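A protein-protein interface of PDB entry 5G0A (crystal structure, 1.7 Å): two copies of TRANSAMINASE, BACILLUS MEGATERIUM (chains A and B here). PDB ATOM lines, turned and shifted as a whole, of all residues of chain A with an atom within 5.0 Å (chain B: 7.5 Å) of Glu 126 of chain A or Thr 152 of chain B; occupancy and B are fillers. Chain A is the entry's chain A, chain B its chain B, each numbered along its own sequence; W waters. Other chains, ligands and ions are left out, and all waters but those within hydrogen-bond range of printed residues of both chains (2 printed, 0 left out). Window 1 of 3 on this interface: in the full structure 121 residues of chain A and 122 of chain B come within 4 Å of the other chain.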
ATOM      1  N   SER A 122     -21.895   0.393  14.515  1.00  0.00           N
ATOM      2  CA  SER A 122     -21.484  -0.294  15.766  1.00  0.00           C
ATOM      3  C   SER A 122     -20.048  -0.729  15.655  1.00  0.00           C
ATOM      4  O   SER A 122     -19.259  -0.571  16.601  1.00  0.00           O
ATOM      5  CB  SER A 122     -22.395  -1.514  16.062  1.00  0.00           C
ATOM      6  OG  SER A 122     -23.684  -1.058  16.418  1.00  0.00           O
ATOM      7  N   GLU A 123     -19.670  -1.264  14.490  1.00  0.00           N
ATOM      8  CA  GLU A 123     -18.289  -1.651  14.281  1.00  0.00           C
ATOM      9  C   GLU A 123     -17.365  -0.420  14.354  1.00  0.00           C
ATOM     10  O   GLU A 123     -16.238  -0.521  14.851  1.00  0.00           O
ATOM     11  CB  GLU A 123     -18.098  -2.399  12.953  1.00  0.00           C
ATOM     12  CG  GLU A 123     -18.619  -3.849  12.995  1.00  0.00           C
ATOM     13  CD  GLU A 123     -18.167  -4.693  11.816  1.00  0.00           C
ATOM     14  OE1 GLU A 123     -17.747  -4.126  10.767  1.00  0.00           O
ATOM     15  OE2 GLU A 123     -18.249  -5.936  11.915  1.00  0.00           O
ATOM     16  N   ALA A 124     -17.834   0.718  13.862  1.00  0.00           N
ATOM     17  CA  ALA A 124     -17.028   1.966  13.971  1.00  0.00           C
ATOM     18  C   ALA A 124     -16.779   2.356  15.423  1.00  0.00           C
ATOM     19  O   ALA A 124     -15.650   2.734  15.822  1.00  0.00           O
ATOM     20  CB  ALA A 124     -17.706   3.108  13.232  1.00  0.00           C
ATOM     21  N   VAL A 125     -17.834   2.249  16.227  1.00  0.00           N
ATOM     22  CA  VAL A 125     -17.736   2.571  17.656  1.00  0.00           C
ATOM     23  C   VAL A 125     -16.769   1.607  18.353  1.00  0.00           C
ATOM     24  O   VAL A 125     -15.937   2.020  19.141  1.00  0.00           O
ATOM     25  CB  VAL A 125     -19.152   2.647  18.315  1.00  0.00           C
ATOM     26  CG1 VAL A 125     -19.051   2.777  19.841  1.00  0.00           C
ATOM     27  CG2 VAL A 125     -19.887   3.865  17.782  1.00  0.00           C
ATOM     28  N   GLU A 126     -16.892   0.326  18.047  1.00  0.00           N
ATOM     29  CA  GLU A 126     -15.990  -0.699  18.584  1.00  0.00           C
ATOM     30  C   GLU A 126     -14.546  -0.315  18.313  1.00  0.00           C
ATOM     31  O   GLU A 126     -13.702  -0.355  19.205  1.00  0.00           O
ATOM     32  CB  GLU A 126     -16.256  -2.065  17.956  1.00  0.00           C
ATOM     33  CG  GLU A 126     -17.627  -2.676  18.267  1.00  0.00           C
ATOM     34  CD  GLU A 126     -17.727  -3.468  19.572  1.00  0.00           C
ATOM     35  OE1 GLU A 126     -16.710  -3.743  20.243  1.00  0.00           O
ATOM     36  OE2 GLU A 126     -18.875  -3.840  19.915  1.00  0.00           O
ATOM     37  N   THR A 127     -14.287   0.060  17.064  1.00  0.00           N
ATOM     38  CA  THR A 127     -12.934   0.387  16.657  1.00  0.00           C
ATOM     39  C   THR A 127     -12.430   1.631  17.400  1.00  0.00           C
ATOM     40  O   THR A 127     -11.288   1.648  17.871  1.00  0.00           O
ATOM     41  CB  THR A 127     -12.906   0.606  15.132  1.00  0.00           C
ATOM     42  OG1 THR A 127     -13.484  -0.540  14.499  1.00  0.00           O
ATOM     43  CG2 THR A 127     -11.475   0.775  14.669  1.00  0.00           C
ATOM     44  N   ALA A 128     -13.269   2.660  17.480  1.00  0.00           N
ATOM     45  CA  ALA A 128     -12.937   3.925  18.198  1.00  0.00           C
ATOM     46  C   ALA A 128     -12.593   3.660  19.695  1.00  0.00           C
ATOM     47  O   ALA A 128     -11.606   4.180  20.232  1.00  0.00           O
ATOM     48  CB  ALA A 128     -14.101   4.914  18.087  1.00  0.00           C
ATOM     49  N   LEU A 129     -13.408   2.832  20.363  1.00  0.00           N
ATOM     50  CA  LEU A 129     -13.167   2.479  21.754  1.00  0.00           C
ATOM     51  C   LEU A 129     -11.817   1.782  21.899  1.00  0.00           C
ATOM     52  O   LEU A 129     -11.054   2.099  22.794  1.00  0.00           O
ATOM     53  CB  LEU A 129     -14.312   1.572  22.283  1.00  0.00           C
ATOM     54  CG  LEU A 129     -15.673   2.281  22.413  1.00  0.00           C
ATOM     55  CD1 LEU A 129     -16.767   1.281  22.832  1.00  0.00           C
ATOM     56  CD2 LEU A 129     -15.600   3.414  23.433  1.00  0.00           C
ATOM     57  N   ASN A 130     -11.531   0.844  20.997  1.00  0.00           N
ATOM     58  CA  ASN A 130     -10.264   0.116  21.004  1.00  0.00           C
ATOM     59  C   ASN A 130      -9.077   1.082  20.817  1.00  0.00           C
ATOM     60  O   ASN A 130      -8.072   1.004  21.551  1.00  0.00           O
ATOM     61  CB  ASN A 130     -10.250  -0.931  19.892  1.00  0.00           C
ATOM     62  CG  ASN A 130     -11.205  -2.106  20.172  1.00  0.00           C
ATOM     63  OD1 ASN A 130     -11.717  -2.231  21.278  1.00  0.00           O
ATOM     64  ND2 ASN A 130     -11.420  -2.972  19.179  1.00  0.00           N
ATOM     65  N   THR A 152     -23.463  -3.902  19.403  1.00  0.00           N
ATOM     66  CA  THR A 152     -22.504  -4.987  19.569  1.00  0.00           C
ATOM     67  C   THR A 152     -21.869  -4.881  20.973  1.00  0.00           C
ATOM     68  O   THR A 152     -22.000  -3.850  21.645  1.00  0.00           O
ATOM     69  CB  THR A 152     -21.458  -4.995  18.441  1.00  0.00           C
ATOM     70  OG1 THR A 152     -20.901  -3.676  18.299  1.00  0.00           O
ATOM     71  CG2 THR A 152     -22.121  -5.401  17.112  1.00  0.00           C
ATOM     72  N   GLY A 153     -21.245  -5.961  21.431  1.00  0.00           N
ATOM     73  CA  GLY A 153     -20.788  -6.054  22.847  1.00  0.00           C
ATOM     74  C   GLY A 153     -20.026  -4.859  23.386  1.00  0.00           C
ATOM     75  O   GLY A 153     -20.328  -4.377  24.468  1.00  0.00           O
ATOM     76  N   GLY A 154     -19.047  -4.353  22.636  1.00  0.00           N
ATOM     77  CA  GLY A 154     -18.293  -3.183  23.091  1.00  0.00           C
ATOM     78  C   GLY A 154     -19.075  -1.880  22.987  1.00  0.00           C
ATOM     79  O   GLY A 154     -19.115  -1.074  23.923  1.00  0.00           O
ATOM     80  N   ALA A 155     -19.680  -1.654  21.823  1.00  0.00           N
ATOM     81  CA  ALA A 155     -20.483  -0.462  21.606  1.00  0.00           C
ATOM     82  C   ALA A 155     -21.655  -0.413  22.568  1.00  0.00           C
ATOM     83  O   ALA A 155     -22.032   0.650  23.022  1.00  0.00           O
ATOM     84  CB  ALA A 155     -20.985  -0.428  20.171  1.00  0.00           C
ATOM     85  N   THR B 120     -21.942  -8.756   9.210  1.00  0.00           N
ATOM     86  CA  THR B 120     -20.620  -9.350   9.314  1.00  0.00           C
ATOM     87  C   THR B 120     -20.629 -10.626  10.171  1.00  0.00           C
ATOM     88  O   THR B 120     -21.585 -10.874  10.903  1.00  0.00           O
ATOM     89  CB  THR B 120     -19.574  -8.373   9.917  1.00  0.00           C
ATOM     90  OG1 THR B 120     -19.847  -8.140  11.312  1.00  0.00           O
ATOM     91  CG2 THR B 120     -19.557  -6.989   9.187  1.00  0.00           C
ATOM     92  N   GLY B 121     -19.548 -11.410  10.079  1.00  0.00           N
ATOM     93  CA  GLY B 121     -19.431 -12.627  10.877  1.00  0.00           C
ATOM     94  C   GLY B 121     -19.338 -12.290  12.360  1.00  0.00           C
ATOM     95  O   GLY B 121     -19.930 -12.984  13.188  1.00  0.00           O
ATOM     96  N   SER B 122     -18.608 -11.216  12.695  1.00  0.00           N
ATOM     97  CA  SER B 122     -18.491 -10.812  14.101  1.00  0.00           C
ATOM     98  C   SER B 122     -19.850 -10.405  14.641  1.00  0.00           C
ATOM     99  O   SER B 122     -20.196 -10.767  15.752  1.00  0.00           O
ATOM    100  CB  SER B 122     -17.506  -9.655  14.295  1.00  0.00           C
ATOM    101  OG  SER B 122     -16.187 -10.097  14.042  1.00  0.00           O
ATOM    102  N   GLU B 123     -20.609  -9.645  13.853  1.00  0.00           N
ATOM    103  CA  GLU B 123     -21.991  -9.304  14.253  1.00  0.00           C
ATOM    104  C   GLU B 123     -22.863 -10.548  14.434  1.00  0.00           C
ATOM    105  O   GLU B 123     -23.702 -10.590  15.334  1.00  0.00           O
ATOM    106  CB  GLU B 123     -22.636  -8.333  13.270  1.00  0.00           C
ATOM    107  CG  GLU B 123     -22.099  -6.896  13.443  1.00  0.00           C
ATOM    108  CD  GLU B 123     -22.877  -5.874  12.634  1.00  0.00           C
ATOM    109  OE1 GLU B 123     -23.627  -6.276  11.715  1.00  0.00           O
ATOM    110  OE2 GLU B 123     -22.763  -4.668  12.952  1.00  0.00           O
ATOM    111  N   ALA B 124     -22.669 -11.552  13.587  1.00  0.00           N
ATOM    112  CA  ALA B 124     -23.419 -12.810  13.747  1.00  0.00           C
ATOM    113  C   ALA B 124     -23.072 -13.498  15.067  1.00  0.00           C
ATOM    114  O   ALA B 124     -23.969 -14.039  15.753  1.00  0.00           O
ATOM    115  CB  ALA B 124     -23.140 -13.767  12.585  1.00  0.00           C
ATOM    116  N   VAL B 125     -21.787 -13.543  15.399  1.00  0.00           N
ATOM    117  CA  VAL B 125     -21.340 -14.134  16.689  1.00  0.00           C
ATOM    118  C   VAL B 125     -21.884 -13.314  17.879  1.00  0.00           C
ATOM    119  O   VAL B 125     -22.370 -13.876  18.850  1.00  0.00           O
ATOM    120  CB  VAL B 125     -19.807 -14.263  16.726  1.00  0.00           C
ATOM    121  CG1 VAL B 125     -19.292 -14.662  18.122  1.00  0.00           C
ATOM    122  CG2 VAL B 125     -19.345 -15.323  15.696  1.00  0.00           C
ATOM    123  N   GLU B 126     -21.837 -11.983  17.785  1.00  0.00           N
ATOM    124  CA  GLU B 126     -22.446 -11.135  18.847  1.00  0.00           C
ATOM    125  C   GLU B 126     -23.897 -11.527  19.077  1.00  0.00           C
ATOM    126  O   GLU B 126     -24.367 -11.661  20.233  1.00  0.00           O
ATOM    127  CB  GLU B 126     -22.370  -9.628  18.509  1.00  0.00           C
ATOM    128  CG  GLU B 126     -20.953  -9.071  18.326  1.00  0.00           C
ATOM    129  CD  GLU B 126     -20.267  -8.708  19.648  1.00  0.00           C
ATOM    130  OE1 GLU B 126     -20.923  -8.699  20.705  1.00  0.00           O
ATOM    131  OE2 GLU B 126     -19.067  -8.417  19.605  1.00  0.00           O
ATOM    132  N   LEU B 129     -24.297 -14.979  20.771  1.00  0.00           N
ATOM    133  CA  LEU B 129     -23.999 -14.932  22.211  1.00  0.00           C
ATOM    134  C   LEU B 129     -25.179 -14.321  22.971  1.00  0.00           C
ATOM    135  O   LEU B 129     -25.587 -14.858  24.001  1.00  0.00           O
ATOM    136  CB  LEU B 129     -22.729 -14.112  22.464  1.00  0.00           C
ATOM    137  CG  LEU B 129     -21.457 -14.746  21.885  1.00  0.00           C
ATOM    138  CD1 LEU B 129     -20.314 -13.734  22.004  1.00  0.00           C
ATOM    139  CD2 LEU B 129     -21.084 -16.097  22.505  1.00  0.00           C
ATOM    140  N   TYR B 148     -10.961 -18.560  17.007  1.00  0.00           N
ATOM    141  CA  TYR B 148     -11.222 -17.212  16.494  1.00  0.00           C
ATOM    142  C   TYR B 148     -12.711 -17.113  16.181  1.00  0.00           C
ATOM    143  O   TYR B 148     -13.248 -17.939  15.425  1.00  0.00           O
ATOM    144  CB  TYR B 148     -10.372 -16.914  15.254  1.00  0.00           C
ATOM    145  CG  TYR B 148     -10.586 -15.473  14.799  1.00  0.00           C
ATOM    146  CD1 TYR B 148      -9.948 -14.423  15.476  1.00  0.00           C
ATOM    147  CD2 TYR B 148     -11.475 -15.160  13.768  1.00  0.00           C
ATOM    148  CE1 TYR B 148     -10.176 -13.095  15.129  1.00  0.00           C
ATOM    149  CE2 TYR B 148     -11.693 -13.821  13.385  1.00  0.00           C
ATOM    150  CZ  TYR B 148     -11.042 -12.803  14.084  1.00  0.00           C
ATOM    151  OH  TYR B 148     -11.236 -11.476  13.754  1.00  0.00           O
ATOM    152  N   HIS B 149     -13.385 -16.134  16.787  1.00  0.00           N
ATOM    153  CA  HIS B 149     -14.802 -15.946  16.574  1.00  0.00           C
ATOM    154  C   HIS B 149     -15.122 -14.503  16.182  1.00  0.00           C
ATOM    155  O   HIS B 149     -16.275 -14.105  16.198  1.00  0.00           O
ATOM    156  CB  HIS B 149     -15.624 -16.382  17.816  1.00  0.00           C
ATOM    157  CG  HIS B 149     -15.520 -17.848  18.104  1.00  0.00           C
ATOM    158  ND1 HIS B 149     -16.026 -18.806  17.247  1.00  0.00           N
ATOM    159  CD2 HIS B 149     -14.965 -18.525  19.144  1.00  0.00           C
ATOM    160  CE1 HIS B 149     -15.767 -20.010  17.738  1.00  0.00           C
ATOM    161  NE2 HIS B 149     -15.134 -19.866  18.892  1.00  0.00           N
ATOM    162  N   GLY B 150     -14.101 -13.723  15.833  1.00  0.00           N
ATOM    163  CA  GLY B 150     -14.378 -12.334  15.434  1.00  0.00           C
ATOM    164  C   GLY B 150     -13.680 -11.332  16.330  1.00  0.00           C
ATOM    165  O   GLY B 150     -12.949 -11.717  17.242  1.00  0.00           O
ATOM    166  N   TRP B 151     -13.936 -10.040  16.095  1.00  0.00           N
ATOM    167  CA  TRP B 151     -13.085  -8.997  16.677  1.00  0.00           C
ATOM    168  C   TRP B 151     -13.809  -7.941  17.516  1.00  0.00           C
ATOM    169  O   TRP B 151     -13.152  -7.191  18.251  1.00  0.00           O
ATOM    170  CB  TRP B 151     -12.282  -8.283  15.573  1.00  0.00           C
ATOM    171  CG  TRP B 151     -13.174  -7.500  14.658  1.00  0.00           C
ATOM    172  CD1 TRP B 151     -13.817  -7.970  13.549  1.00  0.00           C
ATOM    173  CD2 TRP B 151     -13.578  -6.128  14.811  1.00  0.00           C
ATOM    174  NE1 TRP B 151     -14.597  -6.972  12.999  1.00  0.00           N
ATOM    175  CE2 TRP B 151     -14.459  -5.832  13.745  1.00  0.00           C
ATOM    176  CE3 TRP B 151     -13.266  -5.115  15.740  1.00  0.00           C
ATOM    177  CZ2 TRP B 151     -15.034  -4.552  13.565  1.00  0.00           C
ATOM    178  CZ3 TRP B 151     -13.864  -3.848  15.582  1.00  0.00           C
ATOM    179  CH2 TRP B 151     -14.731  -3.581  14.491  1.00  0.00           C
ATOM    180  N   THR B 152     -15.133  -7.837  17.356  1.00  0.00           N
ATOM    181  CA  THR B 152     -15.935  -6.871  18.101  1.00  0.00           C
ATOM    182  C   THR B 152     -15.977  -7.325  19.574  1.00  0.00           C
ATOM    183  O   THR B 152     -15.631  -8.481  19.887  1.00  0.00           O
ATOM    184  CB  THR B 152     -17.363  -6.734  17.498  1.00  0.00           C
ATOM    185  OG1 THR B 152     -17.896  -8.046  17.292  1.00  0.00           O
ATOM    186  CG2 THR B 152     -17.344  -6.017  16.120  1.00  0.00           C
ATOM    187  N   GLY B 153     -16.335  -6.418  20.477  1.00  0.00           N
ATOM    188  CA  GLY B 153     -16.165  -6.638  21.923  1.00  0.00           C
ATOM    189  C   GLY B 153     -16.666  -7.963  22.456  1.00  0.00           C
ATOM    190  O   GLY B 153     -15.934  -8.645  23.168  1.00  0.00           O
ATOM    191  N   GLY B 154     -17.889  -8.358  22.085  1.00  0.00           N
ATOM    192  CA  GLY B 154     -18.437  -9.644  22.536  1.00  0.00           C
ATOM    193  C   GLY B 154     -17.794 -10.862  21.868  1.00  0.00           C
ATOM    194  O   GLY B 154     -17.384 -11.816  22.532  1.00  0.00           O
ATOM    195  N   ALA B 155     -17.681 -10.835  20.539  1.00  0.00           N
ATOM    196  CA  ALA B 155     -17.014 -11.895  19.797  1.00  0.00           C
ATOM    197  C   ALA B 155     -15.540 -12.069  20.227  1.00  0.00           C
ATOM    198  O   ALA B 155     -15.008 -13.167  20.275  1.00  0.00           O
ATOM    199  CB  ALA B 155     -17.095 -11.619  18.299  1.00  0.00           C
ATOM    200  N   ALA B 156     -14.862 -10.963  20.510  1.00  0.00           N
ATOM    201  CA  ALA B 156     -13.477 -11.043  20.979  1.00  0.00           C
ATOM    202  C   ALA B 156     -13.344 -11.766  22.337  1.00  0.00           C
ATOM    203  O   ALA B 156     -12.351 -12.442  22.577  1.00  0.00           O
ATOM    204  CB  ALA B 156     -12.846  -9.654  21.042  1.00  0.00           C
ATOM    205  N   THR B 157     -14.351 -11.663  23.205  1.00  0.00           N
ATOM    206  CA  THR B 157     -14.259 -12.359  24.504  1.00  0.00           C
ATOM    207  C   THR B 157     -14.095 -13.865  24.318  1.00  0.00           C
ATOM    208  O   THR B 157     -13.463 -14.514  25.144  1.00  0.00           O
ATOM    209  CB  THR B 157     -15.450 -12.094  25.464  1.00  0.00           C
ATOM    210  OG1 THR B 157     -16.653 -12.675  24.937  1.00  0.00           O
ATOM    211  CG2 THR B 157     -15.630 -10.563  25.728  1.00  0.00           C
ATOM    212  N   VAL B 158     -14.667 -14.411  23.240  1.00  0.00           N
ATOM    213  CA  VAL B 158     -14.531 -15.849  22.967  1.00  0.00           C
ATOM    214  C   VAL B 158     -13.428 -16.193  21.977  1.00  0.00           C
ATOM    215  O   VAL B 158     -13.221 -17.337  21.626  1.00  0.00           O
ATOM    216  CB  VAL B 158     -15.862 -16.527  22.581  1.00  0.00           C
ATOM    217  CG1 VAL B 158     -16.802 -16.552  23.791  1.00  0.00           C
ATOM    218  CG2 VAL B 158     -16.541 -15.825  21.401  1.00  0.00           C
ATOM    219  N   THR B 159     -12.694 -15.176  21.554  1.00  0.00           N
ATOM    220  CA  THR B 159     -11.535 -15.397  20.708  1.00  0.00           C
ATOM    221  C   THR B 159     -10.324 -15.552  21.614  1.00  0.00           C
ATOM    222  O   THR B 159      -9.973 -14.637  22.367  1.00  0.00           O
ATOM    223  CB  THR B 159     -11.353 -14.212  19.745  1.00  0.00           C
ATOM    224  OG1 THR B 159     -12.392 -14.272  18.758  1.00  0.00           O
ATOM    225  CG2 THR B 159     -10.007 -14.287  19.049  1.00  0.00           C
ATOM    226  N   SER B 166      -6.754  -7.730  18.276  1.00  0.00           N
ATOM    227  CA  SER B 166      -6.768  -6.265  18.071  1.00  0.00           C
ATOM    228  C   SER B 166      -5.868  -5.449  19.002  1.00  0.00           C
ATOM    229  O   SER B 166      -6.098  -4.257  19.218  1.00  0.00           O
ATOM    230  CB  SER B 166      -8.204  -5.730  18.113  1.00  0.00           C
ATOM    231  OG  SER B 166      -9.010  -6.457  17.189  1.00  0.00           O
ATOM    232  N   ILE B 180      -5.673  -4.420  24.631  1.00  0.00           N
ATOM    233  CA  ILE B 180      -6.616  -3.333  24.846  1.00  0.00           C
ATOM    234  C   ILE B 180      -7.069  -3.248  26.318  1.00  0.00           C
ATOM    235  O   ILE B 180      -7.715  -4.167  26.851  1.00  0.00           O
ATOM    236  CB  ILE B 180      -7.872  -3.498  23.960  1.00  0.00           C
ATOM    237  CG1 ILE B 180      -7.483  -3.635  22.473  1.00  0.00           C
ATOM    238  CG2 ILE B 180      -8.837  -2.331  24.161  1.00  0.00           C
ATOM    239  CD1 ILE B 180      -8.636  -4.131  21.611  1.00  0.00           C
HETATM  240  O   HOH W   1     -16.384  -7.487  10.868  1.00  0.00           O
HETATM  241  O   HOH W   2     -13.404  -4.870  19.698  1.00  0.00           O
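The side-chain hydroxyl (OG1) of Thr 127 of chain A sits at hydrogen-bond distance from the backbone carbonyl oxygen (O) of Glu 123 of chain A, at 2.8 Å.
OD1 of Asn 130 of chain A sits close to O of Glu 126 of chain A (3.4 Å).
OE2 of Glu 126 of chain A sits at hydrogen-bond distance from N of Gly 154 of chain A (2.8 Å).
The side-chain carboxylate of Glu 126 of chain A sits at hydrogen-bond distance from the backbone NH of Ala 155 of chain A (3.0 Å).
The backbone NH (N) of Gly 153 of chain B is in hydrogen-bond range of the side-chain carboxylate (OE2) of Glu 126 of chain B, 3.5 Å away.
The backbone carbonyl oxygen of Gly 154 of chain B is in hydrogen-bond range of the side-chain hydroxyl of Thr 157 of chain B, 2.7 Å away.
Of the 13 printed residues of chain A, 7 touch a printed residue of chain B.
Printed residues of chain B that touch a printed residue of chain A: Thr 120, Glu 123, Glu 126, Trp 151, Thr 152, Gly 153, Gly 154 and Ile 180.
Among the printed residues, no Asp or Glu carboxylate lies within 4 Å of a Lys or Arg side-chain nitrogen of the other chain.
OE2 of Glu 123 of chain A is in hydrogen-bond range of OG1 of Thr 120 of chain B.
The side-chain carboxylate (OE1) of Glu 126 of chain A is in hydrogen-bond range of the backbone NH (N) of Gly 153 of chain B (2.7 Å).
The side-chain carboxylate (OE1) of Glu 126 of chain B lies within hydrogen-bond range of the backbone NH (N) of Gly 153 of chain A (2.9 Å).
Ser 122 of chain A touches none of the printed residues of chain B.
Printed residues of chain B within 4 Å of Glu 123 of chain A: Thr 120 and Trp 151.
Printed residues of chain A within 4 Å of Thr 120 of chain B: Glu 123 (2.8 Å).
Printed residues of chain A within 4 Å of Trp 151 of chain B: Glu 123 (3.4 Å), Glu 126 (3.8 Å) and Thr 127 (3.3 Å).
Of the printed residues of chain A, Thr 152 of chain B touches Glu 126 (3.7 Å).
Of the printed residues of chain A, Gly 153 of chain B touches Glu 126 (2.7 Å) and Gly 154 (3.7 Å).
Of the printed residues of chain A, Ile 180 of chain B touches Asn 130 (3.6 Å).
The nearest residue of chain B that does not touch Glu 126 of chain A is Glu 126 of chain B (4.6 Å).
The nearest printed residue of chain A that does not touch Thr 152 of chain B is Glu 123 of chain A (4.01 Å).
The nearest printed residue of chain A that does not touch Ile 180 of chain B is Leu 129 of chain A (5.1 Å).
Among the printed residues, pairs that only touch across the chains: Thr 127 of chain A with Trp 151 of chain B (3.3 Å), Glu 123 of chain A with Trp 151 of chain B (3.4 Å), Asn 130 of chain A with Ile 180 of chain B (3.6 Å), Glu 126 of chain A with Thr 152 of chain B (3.7 Å), Gly 154 of chain A with Gly 153 of chain B (3.7 Å), Gly 153 of chain A with Gly 154 of chain B (3.8 Å), Glu 126 of chain A with Trp 151 of chain B (3.8 Å), Thr 152 of chain A with Glu 126 of chain B (3.9 Å) and Thr 152 of chain A with Glu 123 of chain B (3.96 Å).
Glu 126 of chain A touches Thr 152 of chain B, and with the chains exchanged Thr 152 of chain A touches Glu 126 of chain B.
Glu 126 of chain A touches Gly 153 of chain B, and with the chains exchanged Gly 153 of chain A touches Glu 126 of chain B.
Thr 152 of chain A touches Glu 123 of chain B, but with the chains exchanged Glu 123 of chain A does not touch Thr 152 of chain B (4.01 Å).
Gly 153 of chain A touches Gly 154 of chain B, and with the chains exchanged Gly 154 of chain A touches Gly 153 of chain B.
10 positions are printed for both chains.
Of the 12 pairs that touch across the chains among the printed residues, 6 have their exchanged pair printed and touching as well.
Water W1 lies within hydrogen-bond range of OE2 of Glu 123 of chain A and NE1 of Trp 151 of chain B.
Water W2 lies within hydrogen-bond range of O of Trp 151 of chain B (2.7 Å), ND2 of Asn 130 of chain A (2.8 Å) and N of Gly 153 of chain B (3.4 Å).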
